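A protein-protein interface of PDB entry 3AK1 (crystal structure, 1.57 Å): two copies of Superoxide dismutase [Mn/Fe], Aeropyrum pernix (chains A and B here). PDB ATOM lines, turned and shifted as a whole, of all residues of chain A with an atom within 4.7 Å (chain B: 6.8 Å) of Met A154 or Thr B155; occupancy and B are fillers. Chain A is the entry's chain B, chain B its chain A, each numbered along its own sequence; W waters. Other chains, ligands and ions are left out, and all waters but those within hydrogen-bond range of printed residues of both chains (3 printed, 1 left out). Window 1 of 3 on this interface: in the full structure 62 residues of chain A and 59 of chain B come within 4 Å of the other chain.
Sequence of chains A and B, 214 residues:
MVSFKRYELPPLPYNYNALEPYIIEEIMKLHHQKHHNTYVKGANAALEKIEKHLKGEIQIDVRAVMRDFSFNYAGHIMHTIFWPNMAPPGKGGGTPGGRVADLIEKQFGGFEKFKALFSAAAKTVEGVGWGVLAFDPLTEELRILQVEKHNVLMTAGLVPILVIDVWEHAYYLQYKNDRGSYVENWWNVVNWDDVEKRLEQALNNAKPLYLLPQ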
ATOM      1  N   SER A  70      13.612 -23.830  16.434  1.00  0.00           N
ATOM      2  CA  SER A  70      12.520 -24.783  16.318  1.00  0.00           C
ATOM      3  C   SER A  70      13.034 -26.195  16.542  1.00  0.00           C
ATOM      4  O   SER A  70      12.474 -26.911  17.361  1.00  0.00           O
ATOM      5  CB  SER A  70      11.858 -24.651  14.948  1.00  0.00           C
ATOM      6  OG  SER A  70      11.024 -25.763  14.686  1.00  0.00           O
ATOM      7  N   TYR A  73      14.699 -26.454  20.350  1.00  0.00           N
ATOM      8  CA  TYR A  73      13.657 -26.355  21.375  1.00  0.00           C
ATOM      9  C   TYR A  73      12.778 -27.612  21.383  1.00  0.00           C
ATOM     10  O   TYR A  73      12.493 -28.162  22.443  1.00  0.00           O
ATOM     11  CB  TYR A  73      12.780 -25.106  21.200  1.00  0.00           C
ATOM     12  CG  TYR A  73      11.646 -25.089  22.199  1.00  0.00           C
ATOM     13  CD1 TYR A  73      10.424 -25.700  21.916  1.00  0.00           C
ATOM     14  CD2 TYR A  73      11.805 -24.476  23.440  1.00  0.00           C
ATOM     15  CE1 TYR A  73       9.391 -25.697  22.846  1.00  0.00           C
ATOM     16  CE2 TYR A  73      10.778 -24.460  24.372  1.00  0.00           C
ATOM     17  CZ  TYR A  73       9.577 -25.077  24.078  1.00  0.00           C
ATOM     18  OH  TYR A  73       8.564 -25.045  25.007  1.00  0.00           O
ATOM     19  N   ALA A  74      12.355 -28.061  20.206  1.00  0.00           N
ATOM     20  CA  ALA A  74      11.511 -29.262  20.113  1.00  0.00           C
ATOM     21  C   ALA A  74      12.248 -30.474  20.681  1.00  0.00           C
ATOM     22  O   ALA A  74      11.672 -31.246  21.437  1.00  0.00           O
ATOM     23  CB  ALA A  74      11.085 -29.524  18.691  1.00  0.00           C
ATOM     24  N   LEU A 145      -0.045 -39.607  16.682  1.00  0.00           N
ATOM     25  CA  LEU A 145       0.609 -39.112  15.472  1.00  0.00           C
ATOM     26  C   LEU A 145       2.097 -39.419  15.494  1.00  0.00           C
ATOM     27  O   LEU A 145       2.638 -39.871  16.520  1.00  0.00           O
ATOM     28  CB  LEU A 145       0.368 -37.602  15.298  1.00  0.00           C
ATOM     29  CG  LEU A 145       1.084 -36.629  16.237  1.00  0.00           C
ATOM     30  CD1 LEU A 145       1.079 -35.262  15.589  1.00  0.00           C
ATOM     31  CD2 LEU A 145       0.420 -36.550  17.595  1.00  0.00           C
ATOM     32  N   VAL A 147       5.976 -37.694  14.719  1.00  0.00           N
ATOM     33  CA  VAL A 147       6.777 -36.488  14.504  1.00  0.00           C
ATOM     34  C   VAL A 147       8.086 -36.923  13.857  1.00  0.00           C
ATOM     35  O   VAL A 147       8.703 -37.895  14.298  1.00  0.00           O
ATOM     36  CB  VAL A 147       7.030 -35.737  15.829  1.00  0.00           C
ATOM     37  CG1 VAL A 147       7.989 -34.547  15.621  1.00  0.00           C
ATOM     38  CG2 VAL A 147       5.703 -35.268  16.424  1.00  0.00           C
ATOM     39  N   ASN A 151      10.531 -31.738  14.984  1.00  0.00           N
ATOM     40  CA  ASN A 151       9.757 -30.540  14.673  1.00  0.00           C
ATOM     41  C   ASN A 151       9.104 -30.586  13.301  1.00  0.00           C
ATOM     42  O   ASN A 151       8.905 -29.555  12.670  1.00  0.00           O
ATOM     43  CB  ASN A 151      10.644 -29.275  14.789  1.00  0.00           C
ATOM     44  CG  ASN A 151      11.798 -29.262  13.783  1.00  0.00           C
ATOM     45  OD1 ASN A 151      12.256 -30.315  13.314  1.00  0.00           O
ATOM     46  ND2 ASN A 151      12.288 -28.063  13.466  1.00  0.00           N
ATOM     47  N   VAL A 152       8.755 -31.783  12.837  1.00  0.00           N
ATOM     48  CA  VAL A 152       8.085 -31.941  11.542  1.00  0.00           C
ATOM     49  C   VAL A 152       6.885 -32.835  11.776  1.00  0.00           C
ATOM     50  O   VAL A 152       7.025 -33.902  12.385  1.00  0.00           O
ATOM     51  CB  VAL A 152       9.025 -32.544  10.469  1.00  0.00           C
ATOM     52  CG1 VAL A 152       8.300 -32.734   9.131  1.00  0.00           C
ATOM     53  CG2 VAL A 152      10.233 -31.643  10.270  1.00  0.00           C
ATOM     54  N   LEU A 153       5.715 -32.380  11.319  1.00  0.00           N
ATOM     55  CA  LEU A 153       4.423 -33.063  11.548  1.00  0.00           C
ATOM     56  C   LEU A 153       3.798 -32.770  12.909  1.00  0.00           C
ATOM     57  O   LEU A 153       2.628 -33.100  13.141  1.00  0.00           O
ATOM     58  CB  LEU A 153       4.498 -34.594  11.317  1.00  0.00           C
ATOM     59  CG  LEU A 153       5.101 -35.078   9.997  1.00  0.00           C
ATOM     60  CD1 LEU A 153       5.112 -36.608   9.907  1.00  0.00           C
ATOM     61  CD2 LEU A 153       4.346 -34.461   8.807  1.00  0.00           C
ATOM     62  N   MET A 154       4.562 -32.173  13.819  1.00  0.00           N
ATOM     63  CA  MET A 154       3.970 -31.718  15.067  1.00  0.00           C
ATOM     64  C   MET A 154       3.068 -30.524  14.763  1.00  0.00           C
ATOM     65  O   MET A 154       3.338 -29.738  13.843  1.00  0.00           O
ATOM     66  CB  MET A 154       5.036 -31.375  16.114  1.00  0.00           C
ATOM     67  CG  MET A 154       4.462 -31.108  17.503  1.00  0.00           C
ATOM     68  SD  MET A 154       3.322 -32.398  18.075  1.00  0.00           S
ATOM     69  CE  MET A 154       2.622 -31.648  19.546  1.00  0.00           C
ATOM     70  N   THR A 155       1.976 -30.422  15.505  1.00  0.00           N
ATOM     71  CA  THR A 155       1.005 -29.348  15.320  1.00  0.00           C
ATOM     72  C   THR A 155       0.853 -28.524  16.596  1.00  0.00           C
ATOM     73  O   THR A 155       1.193 -28.980  17.695  1.00  0.00           O
ATOM     74  CB  THR A 155      -0.370 -29.912  14.935  1.00  0.00           C
ATOM     75  OG1 THR A 155      -1.050 -30.356  16.115  1.00  0.00           O
ATOM     76  CG2 THR A 155      -0.242 -31.099  13.940  1.00  0.00           C
ATOM     77  N   ALA A 156       0.334 -27.304  16.457  1.00  0.00           N
ATOM     78  CA  ALA A 156      -0.116 -26.538  17.606  1.00  0.00           C
ATOM     79  C   ALA A 156      -1.254 -27.283  18.309  1.00  0.00           C
ATOM     80  O   ALA A 156      -1.872 -28.192  17.734  1.00  0.00           O
ATOM     81  CB  ALA A 156      -0.589 -25.149  17.148  1.00  0.00           C
ATOM     82  N   LEU A 158      -2.184 -29.831  20.245  1.00  0.00           N
ATOM     83  CA  LEU A 158      -1.965 -31.181  20.788  1.00  0.00           C
ATOM     84  C   LEU A 158      -0.904 -31.198  21.878  1.00  0.00           C
ATOM     85  O   LEU A 158       0.193 -30.676  21.694  1.00  0.00           O
ATOM     86  CB  LEU A 158      -1.599 -32.174  19.674  1.00  0.00           C
ATOM     87  CG  LEU A 158      -2.574 -32.352  18.500  1.00  0.00           C
ATOM     88  CD1 LEU A 158      -2.007 -33.305  17.454  1.00  0.00           C
ATOM     89  CD2 LEU A 158      -3.959 -32.793  18.985  1.00  0.00           C
ATOM     90  N   PRO A 160       1.437 -33.557  23.984  1.00  0.00           N
ATOM     91  CA  PRO A 160       1.981 -34.914  24.136  1.00  0.00           C
ATOM     92  C   PRO A 160       1.948 -35.360  25.609  1.00  0.00           C
ATOM     93  O   PRO A 160       2.401 -34.631  26.492  1.00  0.00           O
ATOM     94  CB  PRO A 160       3.423 -34.782  23.630  1.00  0.00           C
ATOM     95  CG  PRO A 160       3.449 -33.539  22.823  1.00  0.00           C
ATOM     96  CD  PRO A 160       2.434 -32.617  23.429  1.00  0.00           C
ATOM     97  N   SER B  70      -2.219 -34.752  10.647  1.00  0.00           N
ATOM     98  CA  SER B  70      -1.303 -33.699  11.073  1.00  0.00           C
ATOM     99  C   SER B  70      -1.513 -32.403  10.296  1.00  0.00           C
ATOM    100  O   SER B  70      -1.730 -31.357  10.894  1.00  0.00           O
ATOM    101  CB  SER B  70       0.141 -34.163  10.913  1.00  0.00           C
ATOM    102  OG  SER B  70       1.029 -33.073  11.099  1.00  0.00           O
ATOM    103  N   ALA B  74      -3.686 -29.312  11.944  1.00  0.00           N
ATOM    104  CA  ALA B  74      -2.884 -28.114  12.156  1.00  0.00           C
ATOM    105  C   ALA B  74      -3.501 -26.929  11.406  1.00  0.00           C
ATOM    106  O   ALA B  74      -3.572 -25.811  11.933  1.00  0.00           O
ATOM    107  CB  ALA B  74      -1.478 -28.356  11.703  1.00  0.00           C
ATOM    108  N   LEU B 145       8.451 -17.720  16.072  1.00  0.00           N
ATOM    109  CA  LEU B 145       8.929 -18.721  15.113  1.00  0.00           C
ATOM    110  C   LEU B 145       8.109 -18.704  13.831  1.00  0.00           C
ATOM    111  O   LEU B 145       7.097 -17.995  13.736  1.00  0.00           O
ATOM    112  CB  LEU B 145       8.939 -20.132  15.732  1.00  0.00           C
ATOM    113  CG  LEU B 145       7.625 -20.882  15.984  1.00  0.00           C
ATOM    114  CD1 LEU B 145       7.915 -22.380  16.146  1.00  0.00           C
ATOM    115  CD2 LEU B 145       6.889 -20.341  17.210  1.00  0.00           C
ATOM    116  N   VAL B 147       6.175 -21.300  10.952  1.00  0.00           N
ATOM    117  CA  VAL B 147       5.670 -22.612  10.603  1.00  0.00           C
ATOM    118  C   VAL B 147       5.521 -22.677   9.071  1.00  0.00           C
ATOM    119  O   VAL B 147       4.967 -21.757   8.443  1.00  0.00           O
ATOM    120  CB  VAL B 147       4.334 -22.910  11.340  1.00  0.00           C
ATOM    121  CG1 VAL B 147       3.738 -24.232  10.871  1.00  0.00           C
ATOM    122  CG2 VAL B 147       4.523 -22.903  12.860  1.00  0.00           C
ATOM    123  N   HIS B 150       1.226 -26.137   7.588  1.00  0.00           N
ATOM    124  CA  HIS B 150       0.577 -25.879   8.873  1.00  0.00           C
ATOM    125  C   HIS B 150       1.296 -26.612   9.981  1.00  0.00           C
ATOM    126  O   HIS B 150       1.035 -26.376  11.169  1.00  0.00           O
ATOM    127  CB  HIS B 150      -0.877 -26.336   8.855  1.00  0.00           C
ATOM    128  CG  HIS B 150      -1.705 -25.639   7.828  1.00  0.00           C
ATOM    129  ND1 HIS B 150      -2.465 -26.310   6.902  1.00  0.00           N
ATOM    130  CD2 HIS B 150      -1.886 -24.319   7.582  1.00  0.00           C
ATOM    131  CE1 HIS B 150      -3.083 -25.434   6.126  1.00  0.00           C
ATOM    132  NE2 HIS B 150      -2.753 -24.222   6.528  1.00  0.00           N
ATOM    133  N   ASN B 151       2.222 -27.476   9.573  1.00  0.00           N
ATOM    134  CA  ASN B 151       2.690 -28.538  10.446  1.00  0.00           C
ATOM    135  C   ASN B 151       4.151 -28.897  10.257  1.00  0.00           C
ATOM    136  O   ASN B 151       4.547 -30.053  10.431  1.00  0.00           O
ATOM    137  CB  ASN B 151       1.813 -29.784  10.228  1.00  0.00           C
ATOM    138  CG  ASN B 151       1.942 -30.360   8.823  1.00  0.00           C
ATOM    139  OD1 ASN B 151       2.209 -29.639   7.860  1.00  0.00           O
ATOM    140  ND2 ASN B 151       1.738 -31.672   8.697  1.00  0.00           N
ATOM    141  N   VAL B 152       4.967 -27.908   9.902  1.00  0.00           N
ATOM    142  CA  VAL B 152       6.411 -28.110   9.724  1.00  0.00           C
ATOM    143  C   VAL B 152       7.078 -26.962  10.473  1.00  0.00           C
ATOM    144  O   VAL B 152       6.681 -25.800  10.306  1.00  0.00           O
ATOM    145  CB  VAL B 152       6.832 -28.145   8.219  1.00  0.00           C
ATOM    146  CG1 VAL B 152       8.339 -28.303   8.070  1.00  0.00           C
ATOM    147  CG2 VAL B 152       6.096 -29.268   7.449  1.00  0.00           C
ATOM    148  N   LEU B 153       8.056 -27.296  11.312  1.00  0.00           N
ATOM    149  CA  LEU B 153       8.734 -26.359  12.238  1.00  0.00           C
ATOM    150  C   LEU B 153       7.976 -26.045  13.533  1.00  0.00           C
ATOM    151  O   LEU B 153       8.545 -25.497  14.470  1.00  0.00           O
ATOM    152  CB  LEU B 153       9.157 -25.048  11.544  1.00  0.00           C
ATOM    153  CG  LEU B 153       9.995 -25.141  10.257  1.00  0.00           C
ATOM    154  CD1 LEU B 153      10.325 -23.740   9.698  1.00  0.00           C
ATOM    155  CD2 LEU B 153      11.275 -25.993  10.457  1.00  0.00           C
ATOM    156  N   MET B 154       6.691 -26.366  13.590  1.00  0.00           N
ATOM    157  CA  MET B 154       5.955 -26.225  14.831  1.00  0.00           C
ATOM    158  C   MET B 154       6.481 -27.247  15.827  1.00  0.00           C
ATOM    159  O   MET B 154       6.906 -28.330  15.439  1.00  0.00           O
ATOM    160  CB  MET B 154       4.444 -26.383  14.603  1.00  0.00           C
ATOM    161  CG  MET B 154       3.590 -26.006  15.805  1.00  0.00           C
ATOM    162  SD  MET B 154       4.060 -24.420  16.562  1.00  0.00           S
ATOM    163  CE  MET B 154       3.126 -24.524  18.091  1.00  0.00           C
ATOM    164  N   THR B 155       6.479 -26.877  17.105  1.00  0.00           N
ATOM    165  CA  THR B 155       7.013 -27.738  18.159  1.00  0.00           C
ATOM    166  C   THR B 155       5.934 -28.015  19.185  1.00  0.00           C
ATOM    167  O   THR B 155       4.928 -27.294  19.269  1.00  0.00           O
ATOM    168  CB  THR B 155       8.223 -27.087  18.873  1.00  0.00           C
ATOM    169  OG1 THR B 155       7.762 -26.083  19.777  1.00  0.00           O
ATOM    170  CG2 THR B 155       9.201 -26.448  17.865  1.00  0.00           C
ATOM    171  N   ALA B 156       6.140 -29.071  19.968  1.00  0.00           N
ATOM    172  CA  ALA B 156       5.333 -29.293  21.172  1.00  0.00           C
ATOM    173  C   ALA B 156       5.573 -28.155  22.176  1.00  0.00           C
ATOM    174  O   ALA B 156       6.552 -27.408  22.060  1.00  0.00           O
ATOM    175  CB  ALA B 156       5.677 -30.664  21.802  1.00  0.00           C
ATOM    176  N   GLY B 157       4.685 -28.029  23.155  1.00  0.00           N
ATOM    177  CA  GLY B 157       4.864 -27.048  24.232  1.00  0.00           C
ATOM    178  C   GLY B 157       4.354 -25.656  23.918  1.00  0.00           C
ATOM    179  O   GLY B 157       3.381 -25.191  24.527  1.00  0.00           O
ATOM    180  N   LEU B 158       5.033 -24.996  22.976  1.00  0.00           N
ATOM    181  CA  LEU B 158       4.713 -23.631  22.531  1.00  0.00           C
ATOM    182  C   LEU B 158       3.233 -23.407  22.232  1.00  0.00           C
ATOM    183  O   LEU B 158       2.608 -24.176  21.484  1.00  0.00           O
ATOM    184  CB  LEU B 158       5.529 -23.292  21.285  1.00  0.00           C
ATOM    185  CG  LEU B 158       6.886 -22.577  21.335  1.00  0.00           C
ATOM    186  CD1 LEU B 158       7.649 -22.650  22.669  1.00  0.00           C
ATOM    187  CD2 LEU B 158       7.775 -22.949  20.133  1.00  0.00           C
ATOM    188  N   VAL B 159       2.688 -22.343  22.821  1.00  0.00           N
ATOM    189  CA  VAL B 159       1.283 -21.990  22.662  1.00  0.00           C
ATOM    190  C   VAL B 159       1.140 -20.741  21.777  1.00  0.00           C
ATOM    191  O   VAL B 159       1.467 -19.626  22.213  1.00  0.00           O
ATOM    192  CB  VAL B 159       0.593 -21.745  24.044  1.00  0.00           C
ATOM    193  CG1 VAL B 159      -0.905 -21.511  23.848  1.00  0.00           C
ATOM    194  CG2 VAL B 159       0.848 -22.917  25.011  1.00  0.00           C
ATOM    195  N   TYR B 210       3.194 -29.528  31.430  1.00  0.00           N
ATOM    196  CA  TYR B 210       4.503 -30.109  31.204  1.00  0.00           C
ATOM    197  C   TYR B 210       5.293 -30.276  32.498  1.00  0.00           C
ATOM    198  O   TYR B 210       6.137 -31.167  32.574  1.00  0.00           O
ATOM    199  CB  TYR B 210       5.257 -29.299  30.144  1.00  0.00           C
ATOM    200  CG  TYR B 210       4.457 -29.211  28.863  1.00  0.00           C
ATOM    201  CD1 TYR B 210       4.404 -30.289  27.983  1.00  0.00           C
ATOM    202  CD2 TYR B 210       3.708 -28.071  28.555  1.00  0.00           C
ATOM    203  CE1 TYR B 210       3.657 -30.232  26.821  1.00  0.00           C
ATOM    204  CE2 TYR B 210       2.950 -28.007  27.382  1.00  0.00           C
ATOM    205  CZ  TYR B 210       2.930 -29.098  26.532  1.00  0.00           C
ATOM    206  OH  TYR B 210       2.203 -29.060  25.370  1.00  0.00           O
HETATM  207  O   HOH W   1       2.382 -27.765  19.875  1.00  0.00           O
HETATM  208  O   HOH W   2       0.480 -25.932  13.900  1.00  0.00           O
HETATM  209  O   HOH W   3       2.019 -29.081  22.415  1.00  0.00           O
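The backbone carbonyl oxygen (O) of Leu A153 sits at hydrogen-bond distance from the side-chain hydroxyl (OG) of Ser B70, at 2.6 Å.
N of Leu A153 sits at hydrogen-bond distance from O of Asn B151 (2.8 Å).
The side-chain hydroxyl (OG) of Ser A70 sits at hydrogen-bond distance from the backbone carbonyl oxygen (O) of Leu B153 (2.5 Å).
N of Leu B153 is in hydrogen-bond range of O of Asn A151, at 2.8 Å.
The side-chain hydroxyl (OG) of Ser B70 sits at hydrogen-bond distance from the side-chain amide nitrogen (ND2) of Asn B151.
The side-chain hydroxyl (OG) of Ser A70 lies within hydrogen-bond range of the side-chain amide nitrogen (ND2) of Asn A151 (2.9 Å).
Among the printed residues, merely in contact across the chains: Ser A70 with Thr B155 (3.3 Å), Tyr A73 with Thr B155 (3.4 Å), Tyr A73 with Ala B156 (3.4 Å), Tyr A73 with Leu B158 (3.4 Å), Ala A74 with Thr B155 (3.7 Å), Asn A151 with Val B152 (3.9 Å), Asn A151 with Met B154 (3.6 Å), Val A152 with Asn B151 (3.9 Å), Met A154 with Asn B151 (3.6 Å), Met A154 with Met B154 (3.6 Å), Met A154 with Thr B155 (3.8 Å), Met A154 with Ala B156 (3.6 Å), Thr A155 with Ser B70 (3.4 Å), Thr A155 with Ala B74 (3.7 Å), Thr A155 with Met B154 (3.8 Å), Ala A156 with Met B154 (3.6 Å) and Pro A160 with Ala B156 (3.8 Å).
Of the printed residues of chain B, Asn A151 touches Val B152, Leu B153 and Met B154.
Of the printed residues of chain B, Ala A156 touches Met B154 (3.6 Å).
Leu A158 touches none of the printed residues of chain B.
Of chain A, only Ser A70 (3.3 Å), Tyr A73 (3.4 Å), Ala A74 (3.7 Å) and Met A154 (3.8 Å) come within 4 Å of Thr B155.
Gly B157 touches none of the printed residues of chain A.
Printed residues of chain A within 4 Å of Leu B158: Tyr A73 (3.4 Å).
The nearest residue of chain B that does not touch Met A154 is Ser B70 (4.5 Å).
Hydrophobic or aromatic side chains of chain A within 4 Å of the printed part of chain B: Tyr A73, Ala A74, Leu A153, Met A154, Ala A156 and Pro A160.
Of the 15 printed residues of chain B, 9 touch a printed residue of chain A.
Among the printed residues, 21 pairs touch across the chains.
Asn A151 touches Leu B153, and with the chains exchanged Leu A153 touches Asn B151.
Asn A151 touches Met B154, and with the chains exchanged Met A154 touches Asn B151.
Met A154 touches Thr B155, and with the chains exchanged Thr A155 touches Met B154.
Met A154 touches Ala B156, and with the chains exchanged Ala A156 touches Met B154.
Positions printed for both chains: 70, 74, 145, 147, 151, 152, 153, 154, 155, 156 and 158.
Water W3 lies within hydrogen-bond range of O of Leu A158 (2.5 Å), N of Gly B157 (3.0 Å) and OH of Tyr B210 (3.0 Å).
Water W1 bridges the backbone carbonyl oxygen of Thr B155 (2.7 Å) and the backbone carbonyl oxygen of Thr A155 (2.8 Å).
Water W2 bridges O of His B150 and N of Ala A156.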
